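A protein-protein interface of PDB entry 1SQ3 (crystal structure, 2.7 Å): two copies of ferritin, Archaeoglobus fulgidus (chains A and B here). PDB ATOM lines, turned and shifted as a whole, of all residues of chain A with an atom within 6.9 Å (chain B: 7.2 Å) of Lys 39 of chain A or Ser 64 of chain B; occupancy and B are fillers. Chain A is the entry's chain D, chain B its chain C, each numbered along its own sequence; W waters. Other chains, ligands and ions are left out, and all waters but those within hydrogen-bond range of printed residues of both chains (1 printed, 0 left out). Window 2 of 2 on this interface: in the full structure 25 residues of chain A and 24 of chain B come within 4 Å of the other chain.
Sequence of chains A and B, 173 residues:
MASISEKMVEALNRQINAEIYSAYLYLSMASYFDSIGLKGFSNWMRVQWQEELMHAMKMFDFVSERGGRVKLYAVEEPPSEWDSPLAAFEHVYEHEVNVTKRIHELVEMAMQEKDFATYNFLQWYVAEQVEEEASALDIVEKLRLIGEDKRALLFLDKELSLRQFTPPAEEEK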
ATOM      1  N   ALA A  30     -12.249  -9.796  -9.805  1.00  0.00           N
ATOM      2  CA  ALA A  30     -12.298 -10.124 -11.229  1.00  0.00           C
ATOM      3  C   ALA A  30     -13.537  -9.538 -11.852  1.00  0.00           C
ATOM      4  O   ALA A  30     -13.493  -9.096 -13.000  1.00  0.00           O
ATOM      5  CB  ALA A  30     -12.292 -11.583 -11.454  1.00  0.00           C
ATOM      6  N   SER A  31     -14.639  -9.506 -11.106  1.00  0.00           N
ATOM      7  CA  SER A  31     -15.851  -8.908 -11.654  1.00  0.00           C
ATOM      8  C   SER A  31     -15.685  -7.419 -11.789  1.00  0.00           C
ATOM      9  O   SER A  31     -16.090  -6.825 -12.799  1.00  0.00           O
ATOM     10  CB  SER A  31     -17.085  -9.186 -10.803  1.00  0.00           C
ATOM     11  OG  SER A  31     -18.224  -8.629 -11.446  1.00  0.00           O
ATOM     12  N   PHE A  33     -12.960  -5.751 -12.176  1.00  0.00           N
ATOM     13  CA  PHE A  33     -12.093  -5.429 -13.268  1.00  0.00           C
ATOM     14  C   PHE A  33     -12.787  -5.628 -14.608  1.00  0.00           C
ATOM     15  O   PHE A  33     -12.587  -4.789 -15.486  1.00  0.00           O
ATOM     16  CB  PHE A  33     -10.792  -6.211 -13.176  1.00  0.00           C
ATOM     17  CG  PHE A  33      -9.850  -5.685 -12.136  1.00  0.00           C
ATOM     18  CD1 PHE A  33      -9.364  -4.404 -12.226  1.00  0.00           C
ATOM     19  CD2 PHE A  33      -9.406  -6.497 -11.107  1.00  0.00           C
ATOM     20  CE1 PHE A  33      -8.445  -3.946 -11.312  1.00  0.00           C
ATOM     21  CE2 PHE A  33      -8.500  -6.039 -10.191  1.00  0.00           C
ATOM     22  CZ  PHE A  33      -8.038  -4.757 -10.272  1.00  0.00           C
ATOM     23  N   ASP A  34     -13.632  -6.656 -14.768  1.00  0.00           N
ATOM     24  CA  ASP A  34     -14.408  -6.796 -16.018  1.00  0.00           C
ATOM     25  C   ASP A  34     -15.221  -5.521 -16.221  1.00  0.00           C
ATOM     26  O   ASP A  34     -15.418  -5.064 -17.354  1.00  0.00           O
ATOM     27  CB  ASP A  34     -15.436  -7.919 -15.967  1.00  0.00           C
ATOM     28  CG  ASP A  34     -14.856  -9.280 -16.251  1.00  0.00           C
ATOM     29  OD1 ASP A  34     -13.767  -9.394 -16.866  1.00  0.00           O
ATOM     30  OD2 ASP A  34     -15.446 -10.320 -15.863  1.00  0.00           O
ATOM     31  N   SER A  35     -15.793  -5.024 -15.121  1.00  0.00           N
ATOM     32  CA  SER A  35     -16.762  -3.928 -15.183  1.00  0.00           C
ATOM     33  C   SER A  35     -16.109  -2.616 -15.577  1.00  0.00           C
ATOM     34  O   SER A  35     -16.796  -1.682 -15.951  1.00  0.00           O
ATOM     35  CB  SER A  35     -17.499  -3.751 -13.848  1.00  0.00           C
ATOM     36  OG  SER A  35     -16.742  -2.976 -12.939  1.00  0.00           O
ATOM     37  N   ILE A  36     -14.788  -2.529 -15.501  1.00  0.00           N
ATOM     38  CA  ILE A  36     -14.126  -1.355 -16.059  1.00  0.00           C
ATOM     39  C   ILE A  36     -13.210  -1.681 -17.234  1.00  0.00           C
ATOM     40  O   ILE A  36     -12.257  -0.961 -17.461  1.00  0.00           O
ATOM     41  CB  ILE A  36     -13.328  -0.556 -14.979  1.00  0.00           C
ATOM     42  CG1 ILE A  36     -12.223  -1.399 -14.338  1.00  0.00           C
ATOM     43  CG2 ILE A  36     -14.242   0.016 -13.922  1.00  0.00           C
ATOM     44  CD1 ILE A  36     -11.732  -0.773 -13.045  1.00  0.00           C
ATOM     45  N   GLY A  37     -13.473  -2.774 -17.949  1.00  0.00           N
ATOM     46  CA  GLY A  37     -12.728  -3.136 -19.147  1.00  0.00           C
ATOM     47  C   GLY A  37     -11.232  -3.314 -18.969  1.00  0.00           C
ATOM     48  O   GLY A  37     -10.445  -2.880 -19.801  1.00  0.00           O
ATOM     49  N   LEU A  38     -10.835  -4.002 -17.907  1.00  0.00           N
ATOM     50  CA  LEU A  38      -9.457  -4.423 -17.752  1.00  0.00           C
ATOM     51  C   LEU A  38      -9.420  -5.938 -17.684  1.00  0.00           C
ATOM     52  O   LEU A  38      -9.529  -6.522 -16.617  1.00  0.00           O
ATOM     53  CB  LEU A  38      -8.847  -3.761 -16.518  1.00  0.00           C
ATOM     54  CG  LEU A  38      -8.722  -2.240 -16.673  1.00  0.00           C
ATOM     55  CD1 LEU A  38      -8.515  -1.566 -15.319  1.00  0.00           C
ATOM     56  CD2 LEU A  38      -7.603  -1.855 -17.618  1.00  0.00           C
ATOM     57  N   LYS A  39      -9.378  -6.580 -18.840  1.00  0.00           N
ATOM     58  CA  LYS A  39      -9.632  -8.016 -18.897  1.00  0.00           C
ATOM     59  C   LYS A  39      -8.383  -8.750 -18.406  1.00  0.00           C
ATOM     60  O   LYS A  39      -8.454  -9.912 -17.990  1.00  0.00           O
ATOM     61  CB  LYS A  39     -10.035  -8.487 -20.307  1.00  0.00           C
ATOM     62  CG  LYS A  39     -11.425  -8.046 -20.797  1.00  0.00           C
ATOM     63  CD  LYS A  39     -12.561  -9.070 -20.484  1.00  0.00           C
ATOM     64  CE  LYS A  39     -14.011  -8.470 -20.667  1.00  0.00           C
ATOM     65  NZ  LYS A  39     -15.164  -9.284 -20.058  1.00  0.00           N
ATOM     66  N   GLY A  40      -7.258  -8.044 -18.384  1.00  0.00           N
ATOM     67  CA  GLY A  40      -5.997  -8.642 -17.977  1.00  0.00           C
ATOM     68  C   GLY A  40      -5.887  -8.707 -16.470  1.00  0.00           C
ATOM     69  O   GLY A  40      -5.228  -9.588 -15.894  1.00  0.00           O
ATOM     70  N   PHE A  41      -6.488  -7.716 -15.828  1.00  0.00           N
ATOM     71  CA  PHE A  41      -6.479  -7.647 -14.378  1.00  0.00           C
ATOM     72  C   PHE A  41      -7.487  -8.695 -13.925  1.00  0.00           C
ATOM     73  O   PHE A  41      -7.183  -9.558 -13.105  1.00  0.00           O
ATOM     74  CB  PHE A  41      -6.858  -6.256 -13.890  1.00  0.00           C
ATOM     75  CG  PHE A  41      -5.702  -5.260 -13.894  1.00  0.00           C
ATOM     76  CD1 PHE A  41      -5.386  -4.529 -15.040  1.00  0.00           C
ATOM     77  CD2 PHE A  41      -5.029  -4.949 -12.716  1.00  0.00           C
ATOM     78  CE1 PHE A  41      -4.385  -3.583 -15.021  1.00  0.00           C
ATOM     79  CE2 PHE A  41      -4.024  -4.007 -12.710  1.00  0.00           C
ATOM     80  CZ  PHE A  41      -3.716  -3.319 -13.860  1.00  0.00           C
ATOM     81  N   SER A  42      -8.636  -8.702 -14.580  1.00  0.00           N
ATOM     82  CA  SER A  42      -9.589  -9.767 -14.395  1.00  0.00           C
ATOM     83  C   SER A  42      -8.925 -11.152 -14.435  1.00  0.00           C
ATOM     84  O   SER A  42      -9.119 -12.010 -13.554  1.00  0.00           O
ATOM     85  CB  SER A  42     -10.638  -9.658 -15.475  1.00  0.00           C
ATOM     86  OG  SER A  42     -11.774 -10.388 -15.095  1.00  0.00           O
ATOM     87  N   ASN A  43      -8.137 -11.386 -15.472  1.00  0.00           N
ATOM     88  CA  ASN A  43      -7.480 -12.683 -15.623  1.00  0.00           C
ATOM     89  C   ASN A  43      -6.598 -12.968 -14.412  1.00  0.00           C
ATOM     90  O   ASN A  43      -6.626 -14.055 -13.851  1.00  0.00           O
ATOM     91  CB  ASN A  43      -6.629 -12.701 -16.893  1.00  0.00           C
ATOM     92  CG  ASN A  43      -5.838 -13.979 -17.037  1.00  0.00           C
ATOM     93  OD1 ASN A  43      -4.618 -13.986 -16.885  1.00  0.00           O
ATOM     94  ND2 ASN A  43      -6.534 -15.073 -17.328  1.00  0.00           N
ATOM     95  N   TRP A  44      -5.784 -11.987 -14.034  1.00  0.00           N
ATOM     96  CA  TRP A  44      -4.858 -12.158 -12.932  1.00  0.00           C
ATOM     97  C   TRP A  44      -5.612 -12.602 -11.690  1.00  0.00           C
ATOM     98  O   TRP A  44      -5.120 -13.461 -10.949  1.00  0.00           O
ATOM     99  CB  TRP A  44      -4.135 -10.865 -12.645  1.00  0.00           C
ATOM    100  CG  TRP A  44      -3.014 -11.035 -11.702  1.00  0.00           C
ATOM    101  CD1 TRP A  44      -1.701 -11.113 -12.018  1.00  0.00           C
ATOM    102  CD2 TRP A  44      -3.092 -11.109 -10.279  1.00  0.00           C
ATOM    103  NE1 TRP A  44      -0.942 -11.183 -10.877  1.00  0.00           N
ATOM    104  CE2 TRP A  44      -1.772 -11.154  -9.794  1.00  0.00           C
ATOM    105  CE3 TRP A  44      -4.134 -10.997  -9.362  1.00  0.00           C
ATOM    106  CZ2 TRP A  44      -1.463 -11.174  -8.437  1.00  0.00           C
ATOM    107  CZ3 TRP A  44      -3.832 -11.057  -7.998  1.00  0.00           C
ATOM    108  CH2 TRP A  44      -2.504 -11.178  -7.550  1.00  0.00           C
ATOM    109  N   ASP A 157      -2.048  -3.974 -18.046  1.00  0.00           N
ATOM    110  CA  ASP A 157      -3.229  -4.800 -18.156  1.00  0.00           C
ATOM    111  C   ASP A 157      -3.010  -5.939 -19.115  1.00  0.00           C
ATOM    112  O   ASP A 157      -3.429  -7.059 -18.852  1.00  0.00           O
ATOM    113  CB  ASP A 157      -4.426  -3.969 -18.621  1.00  0.00           C
ATOM    114  CG  ASP A 157      -5.651  -4.826 -18.910  1.00  0.00           C
ATOM    115  OD1 ASP A 157      -6.219  -5.442 -17.977  1.00  0.00           O
ATOM    116  OD2 ASP A 157      -6.085  -4.985 -20.065  1.00  0.00           O
ATOM    117  N   LEU A 160      -0.766  -8.584 -17.556  1.00  0.00           N
ATOM    118  CA  LEU A 160      -1.380  -9.374 -16.515  1.00  0.00           C
ATOM    119  C   LEU A 160      -2.258 -10.407 -17.188  1.00  0.00           C
ATOM    120  O   LEU A 160      -2.550 -11.458 -16.626  1.00  0.00           O
ATOM    121  CB  LEU A 160      -2.192  -8.478 -15.583  1.00  0.00           C
ATOM    122  CG  LEU A 160      -1.499  -8.034 -14.286  1.00  0.00           C
ATOM    123  CD1 LEU A 160      -0.033  -7.674 -14.509  1.00  0.00           C
ATOM    124  CD2 LEU A 160      -2.245  -6.877 -13.634  1.00  0.00           C
ATOM    125  N   SER A 161      -2.661 -10.115 -18.412  1.00  0.00           N
ATOM    126  CA  SER A 161      -3.545 -11.018 -19.126  1.00  0.00           C
ATOM    127  C   SER A 161      -2.792 -12.278 -19.592  1.00  0.00           C
ATOM    128  O   SER A 161      -3.420 -13.247 -20.010  1.00  0.00           O
ATOM    129  CB  SER A 161      -4.147 -10.317 -20.327  1.00  0.00           C
ATOM    130  OG  SER A 161      -3.230 -10.415 -21.385  1.00  0.00           O
ATOM    131  N   ILE B   4     -29.522  -7.642 -22.167  1.00  0.00           N
ATOM    132  CA  ILE B   4     -29.768  -8.452 -20.966  1.00  0.00           C
ATOM    133  C   ILE B   4     -30.248  -7.563 -19.822  1.00  0.00           C
ATOM    134  O   ILE B   4     -29.567  -6.615 -19.431  1.00  0.00           O
ATOM    135  CB  ILE B   4     -28.542  -9.254 -20.506  1.00  0.00           C
ATOM    136  CG1 ILE B   4     -28.980 -10.326 -19.493  1.00  0.00           C
ATOM    137  CG2 ILE B   4     -27.531  -8.322 -19.888  1.00  0.00           C
ATOM    138  CD1 ILE B   4     -27.875 -11.212 -18.993  1.00  0.00           C
ATOM    139  N   ASN B  13     -27.213 -14.351 -11.215  1.00  0.00           N
ATOM    140  CA  ASN B  13     -26.257 -14.205 -10.144  1.00  0.00           C
ATOM    141  C   ASN B  13     -26.647 -15.090  -8.957  1.00  0.00           C
ATOM    142  O   ASN B  13     -25.810 -15.796  -8.407  1.00  0.00           O
ATOM    143  CB  ASN B  13     -26.073 -12.739  -9.785  1.00  0.00           C
ATOM    144  CG  ASN B  13     -25.180 -12.027 -10.774  1.00  0.00           C
ATOM    145  OD1 ASN B  13     -24.504 -12.681 -11.547  1.00  0.00           O
ATOM    146  ND2 ASN B  13     -25.149 -10.705 -10.746  1.00  0.00           N
ATOM    147  N   ILE B  16     -25.646 -18.592  -9.932  1.00  0.00           N
ATOM    148  CA  ILE B  16     -24.199 -18.728  -9.781  1.00  0.00           C
ATOM    149  C   ILE B  16     -23.847 -19.103  -8.344  1.00  0.00           C
ATOM    150  O   ILE B  16     -23.040 -20.006  -8.080  1.00  0.00           O
ATOM    151  CB  ILE B  16     -23.500 -17.405 -10.181  1.00  0.00           C
ATOM    152  CG1 ILE B  16     -23.371 -17.326 -11.701  1.00  0.00           C
ATOM    153  CG2 ILE B  16     -22.120 -17.291  -9.541  1.00  0.00           C
ATOM    154  CD1 ILE B  16     -22.703 -16.050 -12.226  1.00  0.00           C
ATOM    155  N   MET B  59     -21.276 -19.686 -16.111  1.00  0.00           N
ATOM    156  CA  MET B  59     -22.324 -18.701 -15.960  1.00  0.00           C
ATOM    157  C   MET B  59     -21.783 -17.326 -15.548  1.00  0.00           C
ATOM    158  O   MET B  59     -22.255 -16.319 -16.068  1.00  0.00           O
ATOM    159  CB  MET B  59     -23.354 -19.193 -14.954  1.00  0.00           C
ATOM    160  CG  MET B  59     -24.632 -18.350 -14.940  1.00  0.00           C
ATOM    161  SD  MET B  59     -26.078 -19.186 -13.918  1.00  0.00           S
ATOM    162  CE  MET B  59     -26.462 -20.738 -14.984  1.00  0.00           C
ATOM    163  N   PHE B  60     -20.800 -17.288 -14.637  1.00  0.00           N
ATOM    164  CA  PHE B  60     -20.022 -16.073 -14.327  1.00  0.00           C
ATOM    165  C   PHE B  60     -19.475 -15.378 -15.580  1.00  0.00           C
ATOM    166  O   PHE B  60     -19.565 -14.153 -15.711  1.00  0.00           O
ATOM    167  CB  PHE B  60     -18.869 -16.409 -13.371  1.00  0.00           C
ATOM    168  CG  PHE B  60     -18.049 -15.212 -12.908  1.00  0.00           C
ATOM    169  CD1 PHE B  60     -17.040 -14.692 -13.698  1.00  0.00           C
ATOM    170  CD2 PHE B  60     -18.181 -14.725 -11.612  1.00  0.00           C
ATOM    171  CE1 PHE B  60     -16.259 -13.645 -13.247  1.00  0.00           C
ATOM    172  CE2 PHE B  60     -17.408 -13.670 -11.169  1.00  0.00           C
ATOM    173  CZ  PHE B  60     -16.448 -13.129 -11.993  1.00  0.00           C
ATOM    174  N   ASP B  61     -18.917 -16.143 -16.509  1.00  0.00           N
ATOM    175  CA  ASP B  61     -18.359 -15.549 -17.723  1.00  0.00           C
ATOM    176  C   ASP B  61     -19.444 -15.034 -18.694  1.00  0.00           C
ATOM    177  O   ASP B  61     -19.248 -14.028 -19.381  1.00  0.00           O
ATOM    178  CB  ASP B  61     -17.492 -16.559 -18.455  1.00  0.00           C
ATOM    179  CG  ASP B  61     -16.163 -16.765 -17.804  1.00  0.00           C
ATOM    180  OD1 ASP B  61     -15.641 -15.851 -17.162  1.00  0.00           O
ATOM    181  OD2 ASP B  61     -15.545 -17.821 -17.913  1.00  0.00           O
ATOM    182  N   PHE B  62     -20.568 -15.747 -18.765  1.00  0.00           N
ATOM    183  CA  PHE B  62     -21.672 -15.386 -19.648  1.00  0.00           C
ATOM    184  C   PHE B  62     -22.335 -14.084 -19.151  1.00  0.00           C
ATOM    185  O   PHE B  62     -22.667 -13.193 -19.930  1.00  0.00           O
ATOM    186  CB  PHE B  62     -22.690 -16.536 -19.686  1.00  0.00           C
ATOM    187  CG  PHE B  62     -23.918 -16.244 -20.503  1.00  0.00           C
ATOM    188  CD1 PHE B  62     -23.859 -16.237 -21.890  1.00  0.00           C
ATOM    189  CD2 PHE B  62     -25.136 -15.976 -19.882  1.00  0.00           C
ATOM    190  CE1 PHE B  62     -24.990 -15.940 -22.655  1.00  0.00           C
ATOM    191  CE2 PHE B  62     -26.258 -15.657 -20.642  1.00  0.00           C
ATOM    192  CZ  PHE B  62     -26.183 -15.639 -22.035  1.00  0.00           C
ATOM    193  N   VAL B  63     -22.513 -13.937 -17.851  1.00  0.00           N
ATOM    194  CA  VAL B  63     -23.071 -12.692 -17.370  1.00  0.00           C
ATOM    195  C   VAL B  63     -22.192 -11.486 -17.742  1.00  0.00           C
ATOM    196  O   VAL B  63     -22.687 -10.509 -18.313  1.00  0.00           O
ATOM    197  CB  VAL B  63     -23.304 -12.737 -15.871  1.00  0.00           C
ATOM    198  CG1 VAL B  63     -23.454 -11.331 -15.337  1.00  0.00           C
ATOM    199  CG2 VAL B  63     -24.529 -13.582 -15.563  1.00  0.00           C
ATOM    200  N   SER B  64     -20.884 -11.586 -17.485  1.00  0.00           N
ATOM    201  CA  SER B  64     -19.932 -10.559 -17.917  1.00  0.00           C
ATOM    202  C   SER B  64     -19.963 -10.356 -19.446  1.00  0.00           C
ATOM    203  O   SER B  64     -20.007  -9.245 -19.915  1.00  0.00           O
ATOM    204  CB  SER B  64     -18.508 -10.908 -17.443  1.00  0.00           C
ATOM    205  OG  SER B  64     -17.518 -10.131 -18.136  1.00  0.00           O
ATOM    206  N   GLU B  65     -19.947 -11.423 -20.235  1.00  0.00           N
ATOM    207  CA  GLU B  65     -19.933 -11.278 -21.690  1.00  0.00           C
ATOM    208  C   GLU B  65     -21.110 -10.459 -22.207  1.00  0.00           C
ATOM    209  O   GLU B  65     -21.020  -9.784 -23.232  1.00  0.00           O
ATOM    210  CB  GLU B  65     -20.062 -12.633 -22.358  1.00  0.00           C
ATOM    211  CG  GLU B  65     -18.799 -13.429 -22.551  1.00  0.00           C
ATOM    212  CD  GLU B  65     -19.186 -14.799 -23.087  1.00  0.00           C
ATOM    213  OE1 GLU B  65     -20.028 -14.795 -24.027  1.00  0.00           O
ATOM    214  OE2 GLU B  65     -18.836 -15.847 -22.463  1.00  0.00           O
ATOM    215  N   ARG B  66     -22.269 -10.739 -21.635  1.00  0.00           N
ATOM    216  CA  ARG B  66     -23.519 -10.123 -22.063  1.00  0.00           C
ATOM    217  C   ARG B  66     -23.629  -8.676 -21.609  1.00  0.00           C
ATOM    218  O   ARG B  66     -24.654  -8.032 -21.842  1.00  0.00           O
ATOM    219  CB  ARG B  66     -24.688 -10.927 -21.510  1.00  0.00           C
ATOM    220  CG  ARG B  66     -24.743 -12.291 -22.135  1.00  0.00           C
ATOM    221  CD  ARG B  66     -25.115 -12.232 -23.589  1.00  0.00           C
ATOM    222  NE  ARG B  66     -26.558 -12.330 -23.688  1.00  0.00           N
ATOM    223  CZ  ARG B  66     -27.406 -11.324 -23.536  1.00  0.00           C
ATOM    224  NH1 ARG B  66     -26.961 -10.075 -23.427  1.00  0.00           N
ATOM    225  NH2 ARG B  66     -28.710 -11.561 -23.597  1.00  0.00           N
ATOM    226  N   GLY B  67     -22.577  -8.201 -20.938  1.00  0.00           N
ATOM    227  CA  GLY B  67     -22.508  -6.842 -20.429  1.00  0.00           C
ATOM    228  C   GLY B  67     -23.122  -6.666 -19.051  1.00  0.00           C
ATOM    229  O   GLY B  67     -23.173  -5.558 -18.543  1.00  0.00           O
ATOM    230  N   GLY B  68     -23.647  -7.745 -18.476  1.00  0.00           N
ATOM    231  CA  GLY B  68     -24.103  -7.762 -17.098  1.00  0.00           C
ATOM    232  C   GLY B  68     -22.983  -7.674 -16.076  1.00  0.00           C
ATOM    233  O   GLY B  68     -21.799  -7.764 -16.386  1.00  0.00           O
ATOM    234  N   ARG B  69     -23.361  -7.474 -14.828  1.00  0.00           N
ATOM    235  CA  ARG B  69     -22.384  -7.414 -13.770  1.00  0.00           C
ATOM    236  C   ARG B  69     -22.625  -8.556 -12.788  1.00  0.00           C
ATOM    237  O   ARG B  69     -23.714  -8.680 -12.226  1.00  0.00           O
ATOM    238  CB  ARG B  69     -22.483  -6.069 -13.060  1.00  0.00           C
ATOM    239  CG  ARG B  69     -21.531  -5.939 -11.891  1.00  0.00           C
ATOM    240  CD  ARG B  69     -20.068  -5.980 -12.276  1.00  0.00           C
ATOM    241  NE  ARG B  69     -19.227  -5.857 -11.094  1.00  0.00           N
ATOM    242  CZ  ARG B  69     -18.987  -4.709 -10.471  1.00  0.00           C
ATOM    243  NH1 ARG B  69     -19.463  -3.562 -10.963  1.00  0.00           N
ATOM    244  NH2 ARG B  69     -18.236  -4.696  -9.376  1.00  0.00           N
ATOM    245  N   VAL B  70     -21.624  -9.417 -12.609  1.00  0.00           N
ATOM    246  CA  VAL B  70     -21.715 -10.426 -11.576  1.00  0.00           C
ATOM    247  C   VAL B  70     -21.522  -9.798 -10.203  1.00  0.00           C
ATOM    248  O   VAL B  70     -20.535  -9.100  -9.974  1.00  0.00           O
ATOM    249  CB  VAL B  70     -20.689 -11.542 -11.739  1.00  0.00           C
ATOM    250  CG1 VAL B  70     -20.758 -12.447 -10.530  1.00  0.00           C
ATOM    251  CG2 VAL B  70     -20.978 -12.344 -12.960  1.00  0.00           C
HETATM  252  O   HOH W   1     -19.013  -9.116 -13.901  1.00  0.00           O
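The side-chain carboxylate (OD2) of Asp 34 of chain A sits at hydrogen-bond distance from the side-chain hydroxyl (OG) of Ser 64 of chain B.
The guanidinium group (NE) of Arg 69 of chain B is in hydrogen-bond range of the side-chain hydroxyl (OG) of Ser 31 of chain A (3.0 Å).
O of Val 70 of chain B sits at hydrogen-bond distance from OG of Ser 31 of chain A (2.8 Å).
The side-chain hydroxyl of Ser 64 of chain B is in hydrogen-bond range of the side-chain amino group of Lys 39 of chain A.
NH1 of Arg 69 of chain B sits at hydrogen-bond distance from OG of Ser 35 of chain A.
The side-chain hydroxyl (OG) of Ser 42 of chain A sits at hydrogen-bond distance from the side-chain carboxylate (OD1) of Asp 34 of chain A (2.8 Å).
NZ of Lys 39 of chain A is in salt-bridge range of OD1 of Asp 34 of chain A (3.5 Å).
The backbone NH (N) of Lys 39 of chain A lies within hydrogen-bond range of the side-chain carboxylate (OD1) of Asp 157 of chain A (3.5 Å).
The backbone carbonyl oxygen of Arg 69 of chain B lies within hydrogen-bond range of the side-chain amide nitrogen of Asn 13 of chain B (2.9 Å).
Of the printed residues of chain B, Ser 31 of chain A touches Arg 69 and Val 70.
Of the printed residues of chain B, Asp 34 of chain A touches Ser 64 (3.1 Å).
Of the printed residues of chain B, Ser 35 of chain A touches Arg 69 (3.4 Å).
Lys 39 of chain A touches just one residue of chain B: Ser 64 (3.2 Å).
Of the printed residues of chain A, Ser 64 of chain B touches Asp 34 and Lys 39.
Of the printed residues of chain A, Arg 69 of chain B touches Ser 31 and Ser 35.
Of the printed residues of chain A, Val 70 of chain B touches Ser 31 (2.8 Å).
The nearest residue of chain B that does not touch Lys 39 of chain A is Glu 65 of chain B (5.2 Å).
The nearest printed residue of chain B that does not touch Ser 31 of chain A is Phe 60 of chain B (4.1 Å).
Printed residues of chain A that touch a printed residue of chain B: Ser 31, Asp 34, Ser 35 and Lys 39.
Of the 15 printed residues of chain B, 3 touch a printed residue of chain A.
Hydrophobic or aromatic side chains of chain B within 4 Å of the printed part of chain A: Val 70.
Among the printed residues, 5 pairs touch across the chains.
Among the printed residues, no Asp or Glu carboxylate lies within 4 Å of a Lys or Arg side-chain nitrogen of the other chain.
No position is printed for both chains.
Water W1 lies within hydrogen-bond range of OG of Ser 31 of chain A (2.6 Å) and N of Val 70 of chain B (2.9 Å).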
